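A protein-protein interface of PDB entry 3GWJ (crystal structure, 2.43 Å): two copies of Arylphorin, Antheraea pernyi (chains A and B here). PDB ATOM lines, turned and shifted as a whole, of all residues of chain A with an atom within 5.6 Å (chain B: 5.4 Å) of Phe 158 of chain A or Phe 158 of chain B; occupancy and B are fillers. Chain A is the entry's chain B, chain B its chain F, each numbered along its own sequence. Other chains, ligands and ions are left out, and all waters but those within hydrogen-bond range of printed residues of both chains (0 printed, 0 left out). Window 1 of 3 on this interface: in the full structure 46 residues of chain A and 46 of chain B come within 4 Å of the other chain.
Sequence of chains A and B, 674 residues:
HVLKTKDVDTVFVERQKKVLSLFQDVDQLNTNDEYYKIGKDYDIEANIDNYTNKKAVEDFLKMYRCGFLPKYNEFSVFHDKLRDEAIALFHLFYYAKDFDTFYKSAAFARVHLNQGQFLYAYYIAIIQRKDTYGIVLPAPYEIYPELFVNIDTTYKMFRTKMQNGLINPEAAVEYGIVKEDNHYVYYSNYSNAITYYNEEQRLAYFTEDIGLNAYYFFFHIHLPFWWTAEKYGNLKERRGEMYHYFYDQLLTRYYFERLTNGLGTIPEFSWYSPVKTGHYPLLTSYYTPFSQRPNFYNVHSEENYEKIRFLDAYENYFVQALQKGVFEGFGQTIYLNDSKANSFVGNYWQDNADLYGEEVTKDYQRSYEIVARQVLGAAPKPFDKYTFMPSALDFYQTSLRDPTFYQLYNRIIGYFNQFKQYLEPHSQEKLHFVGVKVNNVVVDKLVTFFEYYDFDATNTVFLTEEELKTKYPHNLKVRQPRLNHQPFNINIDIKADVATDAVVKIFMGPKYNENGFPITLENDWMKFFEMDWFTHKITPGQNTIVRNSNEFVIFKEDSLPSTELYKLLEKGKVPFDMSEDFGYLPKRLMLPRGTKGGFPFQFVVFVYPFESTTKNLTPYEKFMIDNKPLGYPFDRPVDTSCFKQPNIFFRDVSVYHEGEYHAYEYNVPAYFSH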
ATOM      1  N   THR A 153      -2.129 -20.072  25.454  1.00  0.00           N
ATOM      2  CA  THR A 153      -3.446 -19.528  25.728  1.00  0.00           C
ATOM      3  C   THR A 153      -3.896 -18.656  24.548  1.00  0.00           C
ATOM      4  O   THR A 153      -5.097 -18.562  24.258  1.00  0.00           O
ATOM      5  CB  THR A 153      -3.487 -18.778  27.102  1.00  0.00           C
ATOM      6  OG1 THR A 153      -3.977 -17.443  26.930  1.00  0.00           O
ATOM      7  CG2 THR A 153      -2.138 -18.755  27.732  1.00  0.00           C
ATOM      8  N   THR A 154      -2.942 -18.049  23.844  1.00  0.00           N
ATOM      9  CA  THR A 154      -3.280 -17.249  22.670  1.00  0.00           C
ATOM     10  C   THR A 154      -3.906 -18.159  21.614  1.00  0.00           C
ATOM     11  O   THR A 154      -4.890 -17.787  20.981  1.00  0.00           O
ATOM     12  CB  THR A 154      -2.046 -16.560  22.067  1.00  0.00           C
ATOM     13  OG1 THR A 154      -1.725 -15.405  22.845  1.00  0.00           O
ATOM     14  CG2 THR A 154      -2.313 -16.127  20.639  1.00  0.00           C
ATOM     15  N   TYR A 155      -3.341 -19.353  21.428  1.00  0.00           N
ATOM     16  CA  TYR A 155      -3.884 -20.304  20.458  1.00  0.00           C
ATOM     17  C   TYR A 155      -5.263 -20.818  20.871  1.00  0.00           C
ATOM     18  O   TYR A 155      -6.052 -21.213  20.015  1.00  0.00           O
ATOM     19  CB  TYR A 155      -2.960 -21.508  20.277  1.00  0.00           C
ATOM     20  CG  TYR A 155      -1.691 -21.216  19.517  1.00  0.00           C
ATOM     21  CD1 TYR A 155      -1.556 -20.053  18.770  1.00  0.00           C
ATOM     22  CD2 TYR A 155      -0.628 -22.120  19.522  1.00  0.00           C
ATOM     23  CE1 TYR A 155      -0.405 -19.794  18.047  1.00  0.00           C
ATOM     24  CE2 TYR A 155       0.525 -21.874  18.802  1.00  0.00           C
ATOM     25  CZ  TYR A 155       0.631 -20.709  18.064  1.00  0.00           C
ATOM     26  OH  TYR A 155       1.758 -20.465  17.317  1.00  0.00           O
ATOM     27  N   LYS A 156      -5.544 -20.842  22.173  1.00  0.00           N
ATOM     28  CA  LYS A 156      -6.845 -21.302  22.652  1.00  0.00           C
ATOM     29  C   LYS A 156      -7.882 -20.263  22.271  1.00  0.00           C
ATOM     30  O   LYS A 156      -9.004 -20.605  21.920  1.00  0.00           O
ATOM     31  CB  LYS A 156      -6.841 -21.505  24.172  1.00  0.00           C
ATOM     32  CG  LYS A 156      -6.129 -22.765  24.625  1.00  0.00           C
ATOM     33  CD  LYS A 156      -5.928 -22.779  26.128  1.00  0.00           C
ATOM     34  CE  LYS A 156      -4.996 -23.902  26.548  1.00  0.00           C
ATOM     35  NZ  LYS A 156      -4.754 -23.869  28.022  1.00  0.00           N
ATOM     36  N   MET A 157      -7.502 -18.992  22.348  1.00  0.00           N
ATOM     37  CA  MET A 157      -8.407 -17.922  21.966  1.00  0.00           C
ATOM     38  C   MET A 157      -8.602 -17.981  20.455  1.00  0.00           C
ATOM     39  O   MET A 157      -9.712 -17.776  19.965  1.00  0.00           O
ATOM     40  CB  MET A 157      -7.854 -16.553  22.372  1.00  0.00           C
ATOM     41  CG  MET A 157      -7.802 -16.346  23.879  1.00  0.00           C
ATOM     42  SD  MET A 157      -7.488 -14.636  24.368  1.00  0.00           S
ATOM     43  CE  MET A 157      -5.708 -14.660  24.586  1.00  0.00           C
ATOM     44  N   PHE A 158      -7.532 -18.263  19.715  1.00  0.00           N
ATOM     45  CA  PHE A 158      -7.634 -18.366  18.263  1.00  0.00           C
ATOM     46  C   PHE A 158      -8.603 -19.465  17.886  1.00  0.00           C
ATOM     47  O   PHE A 158      -9.411 -19.300  16.974  1.00  0.00           O
ATOM     48  CB  PHE A 158      -6.280 -18.694  17.618  1.00  0.00           C
ATOM     49  CG  PHE A 158      -5.343 -17.529  17.529  1.00  0.00           C
ATOM     50  CD1 PHE A 158      -5.780 -16.235  17.805  1.00  0.00           C
ATOM     51  CD2 PHE A 158      -4.014 -17.726  17.175  1.00  0.00           C
ATOM     52  CE1 PHE A 158      -4.905 -15.160  17.735  1.00  0.00           C
ATOM     53  CE2 PHE A 158      -3.130 -16.656  17.101  1.00  0.00           C
ATOM     54  CZ  PHE A 158      -3.573 -15.372  17.382  1.00  0.00           C
ATOM     55  N   ARG A 159      -8.506 -20.592  18.582  1.00  0.00           N
ATOM     56  CA  ARG A 159      -9.372 -21.725  18.296  1.00  0.00           C
ATOM     57  C   ARG A 159     -10.826 -21.320  18.490  1.00  0.00           C
ATOM     58  O   ARG A 159     -11.664 -21.520  17.608  1.00  0.00           O
ATOM     59  CB  ARG A 159      -9.045 -22.905  19.211  1.00  0.00           C
ATOM     60  CG  ARG A 159      -9.596 -24.222  18.704  1.00  0.00           C
ATOM     61  CD  ARG A 159      -9.865 -25.200  19.832  1.00  0.00           C
ATOM     62  NE  ARG A 159      -8.681 -25.450  20.643  1.00  0.00           N
ATOM     63  CZ  ARG A 159      -8.708 -26.029  21.840  1.00  0.00           C
ATOM     64  NH1 ARG A 159      -7.574 -26.221  22.514  1.00  0.00           N
ATOM     65  NH2 ARG A 159      -9.873 -26.410  22.369  1.00  0.00           N
ATOM     66  N   THR A 160     -11.116 -20.724  19.645  1.00  0.00           N
ATOM     67  CA  THR A 160     -12.473 -20.304  19.966  1.00  0.00           C
ATOM     68  C   THR A 160     -13.055 -19.366  18.925  1.00  0.00           C
ATOM     69  O   THR A 160     -14.201 -19.507  18.536  1.00  0.00           O
ATOM     70  CB  THR A 160     -12.539 -19.593  21.323  1.00  0.00           C
ATOM     71  OG1 THR A 160     -12.009 -20.449  22.341  1.00  0.00           O
ATOM     72  CG2 THR A 160     -13.988 -19.239  21.658  1.00  0.00           C
ATOM     73  N   LYS A 161     -12.261 -18.405  18.475  1.00  0.00           N
ATOM     74  CA  LYS A 161     -12.737 -17.449  17.494  1.00  0.00           C
ATOM     75  C   LYS A 161     -13.029 -18.143  16.162  1.00  0.00           C
ATOM     76  O   LYS A 161     -14.034 -17.847  15.512  1.00  0.00           O
ATOM     77  CB  LYS A 161     -11.708 -16.336  17.301  1.00  0.00           C
ATOM     78  CG  LYS A 161     -12.232 -15.126  16.533  1.00  0.00           C
ATOM     79  CD  LYS A 161     -13.452 -14.534  17.242  1.00  0.00           C
ATOM     80  CE  LYS A 161     -13.957 -13.260  16.568  1.00  0.00           C
ATOM     81  NZ  LYS A 161     -14.412 -13.470  15.161  1.00  0.00           N
ATOM     82  N   MET A 162     -12.160 -19.075  15.773  1.00  0.00           N
ATOM     83  CA  MET A 162     -12.329 -19.803  14.519  1.00  0.00           C
ATOM     84  C   MET A 162     -13.559 -20.691  14.565  1.00  0.00           C
ATOM     85  O   MET A 162     -14.269 -20.821  13.573  1.00  0.00           O
ATOM     86  CB  MET A 162     -11.085 -20.651  14.209  1.00  0.00           C
ATOM     87  CG  MET A 162      -9.860 -19.840  13.792  1.00  0.00           C
ATOM     88  SD  MET A 162      -8.468 -20.858  13.217  1.00  0.00           S
ATOM     89  CE  MET A 162      -7.512 -21.061  14.754  1.00  0.00           C
ATOM     90  N   GLN A 163     -13.816 -21.292  15.723  1.00  0.00           N
ATOM     91  CA  GLN A 163     -14.975 -22.160  15.875  1.00  0.00           C
ATOM     92  C   GLN A 163     -16.224 -21.315  16.129  1.00  0.00           C
ATOM     93  O   GLN A 163     -17.348 -21.810  16.068  1.00  0.00           O
ATOM     94  CB  GLN A 163     -14.778 -23.116  17.053  1.00  0.00           C
ATOM     95  CG  GLN A 163     -13.503 -23.928  17.029  1.00  0.00           C
ATOM     96  CD  GLN A 163     -13.454 -24.912  18.178  1.00  0.00           C
ATOM     97  OE1 GLN A 163     -13.880 -24.597  19.283  1.00  0.00           O
ATOM     98  NE2 GLN A 163     -12.931 -26.109  17.928  1.00  0.00           N
ATOM     99  N   THR A 460      -6.534  -9.880  21.032  1.00  0.00           N
ATOM    100  CA  THR A 460      -5.776 -11.023  20.522  1.00  0.00           C
ATOM    101  C   THR A 460      -6.326 -11.564  19.206  1.00  0.00           C
ATOM    102  O   THR A 460      -5.580 -11.968  18.317  1.00  0.00           O
ATOM    103  CB  THR A 460      -5.802 -12.181  21.527  1.00  0.00           C
ATOM    104  OG1 THR A 460      -5.193 -11.765  22.754  1.00  0.00           O
ATOM    105  CG2 THR A 460      -5.059 -13.379  20.967  1.00  0.00           C
ATOM    106  N   VAL A 461      -7.650 -11.564  19.127  1.00  0.00           N
ATOM    107  CA  VAL A 461      -8.440 -12.068  18.009  1.00  0.00           C
ATOM    108  C   VAL A 461      -8.807 -11.033  16.924  1.00  0.00           C
ATOM    109  O   VAL A 461      -8.697  -9.821  17.137  1.00  0.00           O
ATOM    110  CB  VAL A 461      -9.728 -12.694  18.612  1.00  0.00           C
ATOM    111  CG1 VAL A 461     -10.904 -12.518  17.702  1.00  0.00           C
ATOM    112  CG2 VAL A 461      -9.478 -14.147  18.924  1.00  0.00           C
ATOM    113  N   PHE A 462      -9.226 -11.522  15.756  1.00  0.00           N
ATOM    114  CA  PHE A 462      -9.660 -10.651  14.655  1.00  0.00           C
ATOM    115  C   PHE A 462     -11.178 -10.742  14.516  1.00  0.00           C
ATOM    116  O   PHE A 462     -11.759 -11.819  14.677  1.00  0.00           O
ATOM    117  CB  PHE A 462      -9.027 -11.054  13.324  1.00  0.00           C
ATOM    118  CG  PHE A 462      -7.565 -10.795  13.253  1.00  0.00           C
ATOM    119  CD1 PHE A 462      -6.661 -11.677  13.836  1.00  0.00           C
ATOM    120  CD2 PHE A 462      -7.086  -9.654  12.625  1.00  0.00           C
ATOM    121  CE1 PHE A 462      -5.304 -11.424  13.795  1.00  0.00           C
ATOM    122  CE2 PHE A 462      -5.728  -9.395  12.581  1.00  0.00           C
ATOM    123  CZ  PHE A 462      -4.834 -10.283  13.167  1.00  0.00           C
ATOM    124  N   THR B 153       2.453 -18.145   7.272  1.00  0.00           N
ATOM    125  CA  THR B 153       1.297 -18.429   6.425  1.00  0.00           C
ATOM    126  C   THR B 153       0.203 -19.109   7.258  1.00  0.00           C
ATOM    127  O   THR B 153      -0.986 -18.947   6.988  1.00  0.00           O
ATOM    128  CB  THR B 153       1.675 -19.272   5.165  1.00  0.00           C
ATOM    129  OG1 THR B 153       0.833 -20.424   5.079  1.00  0.00           O
ATOM    130  CG2 THR B 153       3.130 -19.675   5.197  1.00  0.00           C
ATOM    131  N   THR B 154       0.602 -19.845   8.289  1.00  0.00           N
ATOM    132  CA  THR B 154      -0.374 -20.470   9.176  1.00  0.00           C
ATOM    133  C   THR B 154      -1.195 -19.349   9.846  1.00  0.00           C
ATOM    134  O   THR B 154      -2.424 -19.424   9.959  1.00  0.00           O
ATOM    135  CB  THR B 154       0.324 -21.294  10.281  1.00  0.00           C
ATOM    136  OG1 THR B 154       0.858 -22.494   9.715  1.00  0.00           O
ATOM    137  CG2 THR B 154      -0.656 -21.650  11.400  1.00  0.00           C
ATOM    138  N   TYR B 155      -0.502 -18.304  10.282  1.00  0.00           N
ATOM    139  CA  TYR B 155      -1.171 -17.193  10.929  1.00  0.00           C
ATOM    140  C   TYR B 155      -2.106 -16.458   9.986  1.00  0.00           C
ATOM    141  O   TYR B 155      -3.104 -15.895  10.427  1.00  0.00           O
ATOM    142  CB  TYR B 155      -0.149 -16.227  11.518  1.00  0.00           C
ATOM    143  CG  TYR B 155       0.458 -16.712  12.816  1.00  0.00           C
ATOM    144  CD1 TYR B 155       0.048 -17.916  13.396  1.00  0.00           C
ATOM    145  CD2 TYR B 155       1.446 -15.973  13.466  1.00  0.00           C
ATOM    146  CE1 TYR B 155       0.609 -18.372  14.589  1.00  0.00           C
ATOM    147  CE2 TYR B 155       2.011 -16.422  14.662  1.00  0.00           C
ATOM    148  CZ  TYR B 155       1.586 -17.619  15.212  1.00  0.00           C
ATOM    149  OH  TYR B 155       2.140 -18.062  16.381  1.00  0.00           O
ATOM    150  N   LYS B 156      -1.788 -16.456   8.694  1.00  0.00           N
ATOM    151  CA  LYS B 156      -2.650 -15.788   7.730  1.00  0.00           C
ATOM    152  C   LYS B 156      -3.936 -16.586   7.586  1.00  0.00           C
ATOM    153  O   LYS B 156      -5.015 -16.014   7.463  1.00  0.00           O
ATOM    154  CB  LYS B 156      -1.949 -15.629   6.382  1.00  0.00           C
ATOM    155  CG  LYS B 156      -0.855 -14.574   6.417  1.00  0.00           C
ATOM    156  CD  LYS B 156       0.004 -14.579   5.164  1.00  0.00           C
ATOM    157  CE  LYS B 156       1.234 -13.697   5.377  1.00  0.00           C
ATOM    158  NZ  LYS B 156       2.149 -13.665   4.204  1.00  0.00           N
ATOM    159  N   MET B 157      -3.832 -17.909   7.615  1.00  0.00           N
ATOM    160  CA  MET B 157      -5.037 -18.719   7.525  1.00  0.00           C
ATOM    161  C   MET B 157      -5.886 -18.484   8.785  1.00  0.00           C
ATOM    162  O   MET B 157      -7.109 -18.327   8.691  1.00  0.00           O
ATOM    163  CB  MET B 157      -4.686 -20.201   7.368  1.00  0.00           C
ATOM    164  CG  MET B 157      -4.108 -20.521   6.009  1.00  0.00           C
ATOM    165  SD  MET B 157      -3.738 -22.260   5.750  1.00  0.00           S
ATOM    166  CE  MET B 157      -2.002 -22.267   6.064  1.00  0.00           C
ATOM    167  N   PHE B 158      -5.229 -18.441   9.949  1.00  0.00           N
ATOM    168  CA  PHE B 158      -5.920 -18.206  11.218  1.00  0.00           C
ATOM    169  C   PHE B 158      -6.678 -16.884  11.169  1.00  0.00           C
ATOM    170  O   PHE B 158      -7.831 -16.809  11.594  1.00  0.00           O
ATOM    171  CB  PHE B 158      -4.934 -18.150  12.393  1.00  0.00           C
ATOM    172  CG  PHE B 158      -4.437 -19.495  12.859  1.00  0.00           C
ATOM    173  CD1 PHE B 158      -4.836 -20.667  12.235  1.00  0.00           C
ATOM    174  CD2 PHE B 158      -3.522 -19.574  13.904  1.00  0.00           C
ATOM    175  CE1 PHE B 158      -4.328 -21.900  12.642  1.00  0.00           C
ATOM    176  CE2 PHE B 158      -3.008 -20.802  14.318  1.00  0.00           C
ATOM    177  CZ  PHE B 158      -3.413 -21.969  13.683  1.00  0.00           C
ATOM    178  N   ARG B 159      -6.024 -15.845  10.655  1.00  0.00           N
ATOM    179  CA  ARG B 159      -6.654 -14.536  10.562  1.00  0.00           C
ATOM    180  C   ARG B 159      -7.843 -14.570   9.600  1.00  0.00           C
ATOM    181  O   ARG B 159      -8.828 -13.871   9.807  1.00  0.00           O
ATOM    182  CB  ARG B 159      -5.655 -13.483  10.087  1.00  0.00           C
ATOM    183  CG  ARG B 159      -6.111 -12.047  10.350  1.00  0.00           C
ATOM    184  CD  ARG B 159      -5.643 -11.100   9.260  1.00  0.00           C
ATOM    185  NE  ARG B 159      -4.207 -11.196   9.010  1.00  0.00           N
ATOM    186  CZ  ARG B 159      -3.621 -10.808   7.877  1.00  0.00           C
ATOM    187  NH1 ARG B 159      -2.300 -10.926   7.729  1.00  0.00           N
ATOM    188  NH2 ARG B 159      -4.360 -10.314   6.883  1.00  0.00           N
ATOM    189  N   THR B 160      -7.756 -15.386   8.555  1.00  0.00           N
ATOM    190  CA  THR B 160      -8.835 -15.477   7.587  1.00  0.00           C
ATOM    191  C   THR B 160     -10.052 -16.152   8.189  1.00  0.00           C
ATOM    192  O   THR B 160     -11.174 -15.668   8.048  1.00  0.00           O
ATOM    193  CB  THR B 160      -8.404 -16.255   6.339  1.00  0.00           C
ATOM    194  OG1 THR B 160      -7.320 -15.569   5.705  1.00  0.00           O
ATOM    195  CG2 THR B 160      -9.558 -16.364   5.352  1.00  0.00           C
ATOM    196  N   LYS B 161      -9.822 -17.267   8.866  1.00  0.00           N
ATOM    197  CA  LYS B 161     -10.898 -18.021   9.497  1.00  0.00           C
ATOM    198  C   LYS B 161     -11.545 -17.212  10.615  1.00  0.00           C
ATOM    199  O   LYS B 161     -12.761 -17.280  10.809  1.00  0.00           O
ATOM    200  CB  LYS B 161     -10.358 -19.332  10.066  1.00  0.00           C
ATOM    201  CG  LYS B 161     -11.430 -20.318  10.456  1.00  0.00           C
ATOM    202  CD  LYS B 161     -12.227 -20.740   9.231  1.00  0.00           C
ATOM    203  CE  LYS B 161     -13.222 -21.818   9.580  1.00  0.00           C
ATOM    204  NZ  LYS B 161     -14.143 -21.320  10.633  1.00  0.00           N
ATOM    205  N   MET B 162     -10.733 -16.463  11.362  1.00  0.00           N
ATOM    206  CA  MET B 162     -11.252 -15.634  12.451  1.00  0.00           C
ATOM    207  C   MET B 162     -12.120 -14.503  11.903  1.00  0.00           C
ATOM    208  O   MET B 162     -13.138 -14.154  12.490  1.00  0.00           O
ATOM    209  CB  MET B 162     -10.113 -15.043  13.291  1.00  0.00           C
ATOM    210  CG  MET B 162      -9.502 -16.016  14.304  1.00  0.00           C
ATOM    211  SD  MET B 162      -8.377 -15.205  15.484  1.00  0.00           S
ATOM    212  CE  MET B 162      -6.795 -15.343  14.616  1.00  0.00           C
ATOM    213  N   GLN B 163     -11.708 -13.928  10.780  1.00  0.00           N
ATOM    214  CA  GLN B 163     -12.468 -12.850  10.164  1.00  0.00           C
ATOM    215  C   GLN B 163     -13.603 -13.452   9.354  1.00  0.00           C
ATOM    216  O   GLN B 163     -14.475 -12.739   8.872  1.00  0.00           O
ATOM    217  CB  GLN B 163     -11.584 -12.019   9.229  1.00  0.00           C
ATOM    218  CG  GLN B 163     -10.413 -11.321   9.887  1.00  0.00           C
ATOM    219  CD  GLN B 163      -9.602 -10.536   8.878  1.00  0.00           C
ATOM    220  OE1 GLN B 163      -9.421 -10.983   7.742  1.00  0.00           O
ATOM    221  NE2 GLN B 163      -9.106  -9.366   9.280  1.00  0.00           N
ATOM    222  N   THR B 460      -5.443 -26.821   8.833  1.00  0.00           N
ATOM    223  CA  THR B 460      -4.778 -25.814   9.658  1.00  0.00           C
ATOM    224  C   THR B 460      -5.783 -25.096  10.559  1.00  0.00           C
ATOM    225  O   THR B 460      -5.477 -24.689  11.678  1.00  0.00           O
ATOM    226  CB  THR B 460      -4.118 -24.734   8.771  1.00  0.00           C
ATOM    227  OG1 THR B 460      -3.157 -25.344   7.912  1.00  0.00           O
ATOM    228  CG2 THR B 460      -3.432 -23.677   9.615  1.00  0.00           C
ATOM    229  N   VAL B 461      -6.991 -24.960  10.042  1.00  0.00           N
ATOM    230  CA  VAL B 461      -8.070 -24.242  10.698  1.00  0.00           C
ATOM    231  C   VAL B 461      -9.119 -25.068  11.462  1.00  0.00           C
ATOM    232  O   VAL B 461      -9.277 -26.260  11.231  1.00  0.00           O
ATOM    233  CB  VAL B 461      -8.753 -23.371   9.627  1.00  0.00           C
ATOM    234  CG1 VAL B 461     -10.189 -23.152   9.954  1.00  0.00           C
ATOM    235  CG2 VAL B 461      -8.014 -22.056   9.498  1.00  0.00           C
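Thr 153 of chain A touches none of the printed residues of chain B.
Printed residues of chain B within 4 Å of Lys 161 of chain A: Met 162 (3.0 Å).
Printed residues of chain B within 4 Å of Val 461 of chain A: Met 162.
Of chain A, only Phe 158 and Met 162 come within 4 Å of Phe 158 of chain B.
Thr 460 of chain B touches none of the printed residues of chain A.
The nearest printed residue of chain B that does not touch Met 162 of chain A is Thr 460 of chain B (5.1 Å).
Tyr 155 of chain A touches its own counterpart, Tyr 155 of chain B.
Phe 158 of chain B touches its own counterpart, Phe 158 of chain A.
Lys 161 of chain A touches Met 162 of chain B, and with the chains exchanged Met 162 of chain A touches Lys 161 of chain B.
Met 162 of chain A touches its own counterpart, Met 162 of chain B.
Of the 12 pairs that touch across the chains among the printed residues, 9 have their exchanged pair printed and touching as well.
Phe 158 of chain B touches Phe 158 of chain A (CD2 to CD2, 3.8 Å).
Met 162 of chain B touches Phe 158 of chain A (CE to CD1, 3.5 Å).
Met 162 of chain A touches Phe 158 of chain B.
Met 162 of chain A touches Met 162 of chain B (CG to CG, 3.9 Å).
Val 461 of chain B touches Met 162 of chain A.
SD of Met 162 of chain B touches CG2 of Val 461 of chain A, at 3.8 Å.
Phe 462 of chain A touches Arg 159 of chain B (CD2 to CG, 3.4 Å).
Phe 462 of chain A touches Gln 163 of chain B.
Printed residues of chain B that touch a printed residue of chain A: Tyr 155, Phe 158, Arg 159, Lys 161, Met 162, Gln 163 and Val 461.
Hydrophobic or aromatic side chains of chain B within 4 Å of the printed part of chain A: Tyr 155, Phe 158, Met 162 and Val 461.
Of the 14 printed residues of chain A, 6 touch a printed residue of chain B.
Printed residues of chain A that touch a printed residue of chain B: Tyr 155, Phe 158, Lys 161, Met 162, Val 461 and Phe 462.
Hydrophobic or aromatic side chains of chain A that line the printed part of chain B: Tyr 155, Phe 158, Met 162, Val 461 and Phe 462.
The side-chain hydroxyl of Tyr 155 of chain B sits at hydrogen-bond distance from the side-chain hydroxyl of Tyr 155 of chain A (2.6 Å).
O of Met 162 of chain B lies within hydrogen-bond range of NZ of Lys 161 of chain A (3.0 Å).
O of Met 162 of chain A sits at hydrogen-bond distance from NZ of Lys 161 of chain B.
N of Phe 462 of chain A sits at hydrogen-bond distance from SD of Met 162 of chain B.
The side-chain amino group (NZ) of Lys 161 of chain A lies within hydrogen-bond range of the backbone carbonyl oxygen (O) of Phe 462 of chain A (3.2 Å).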
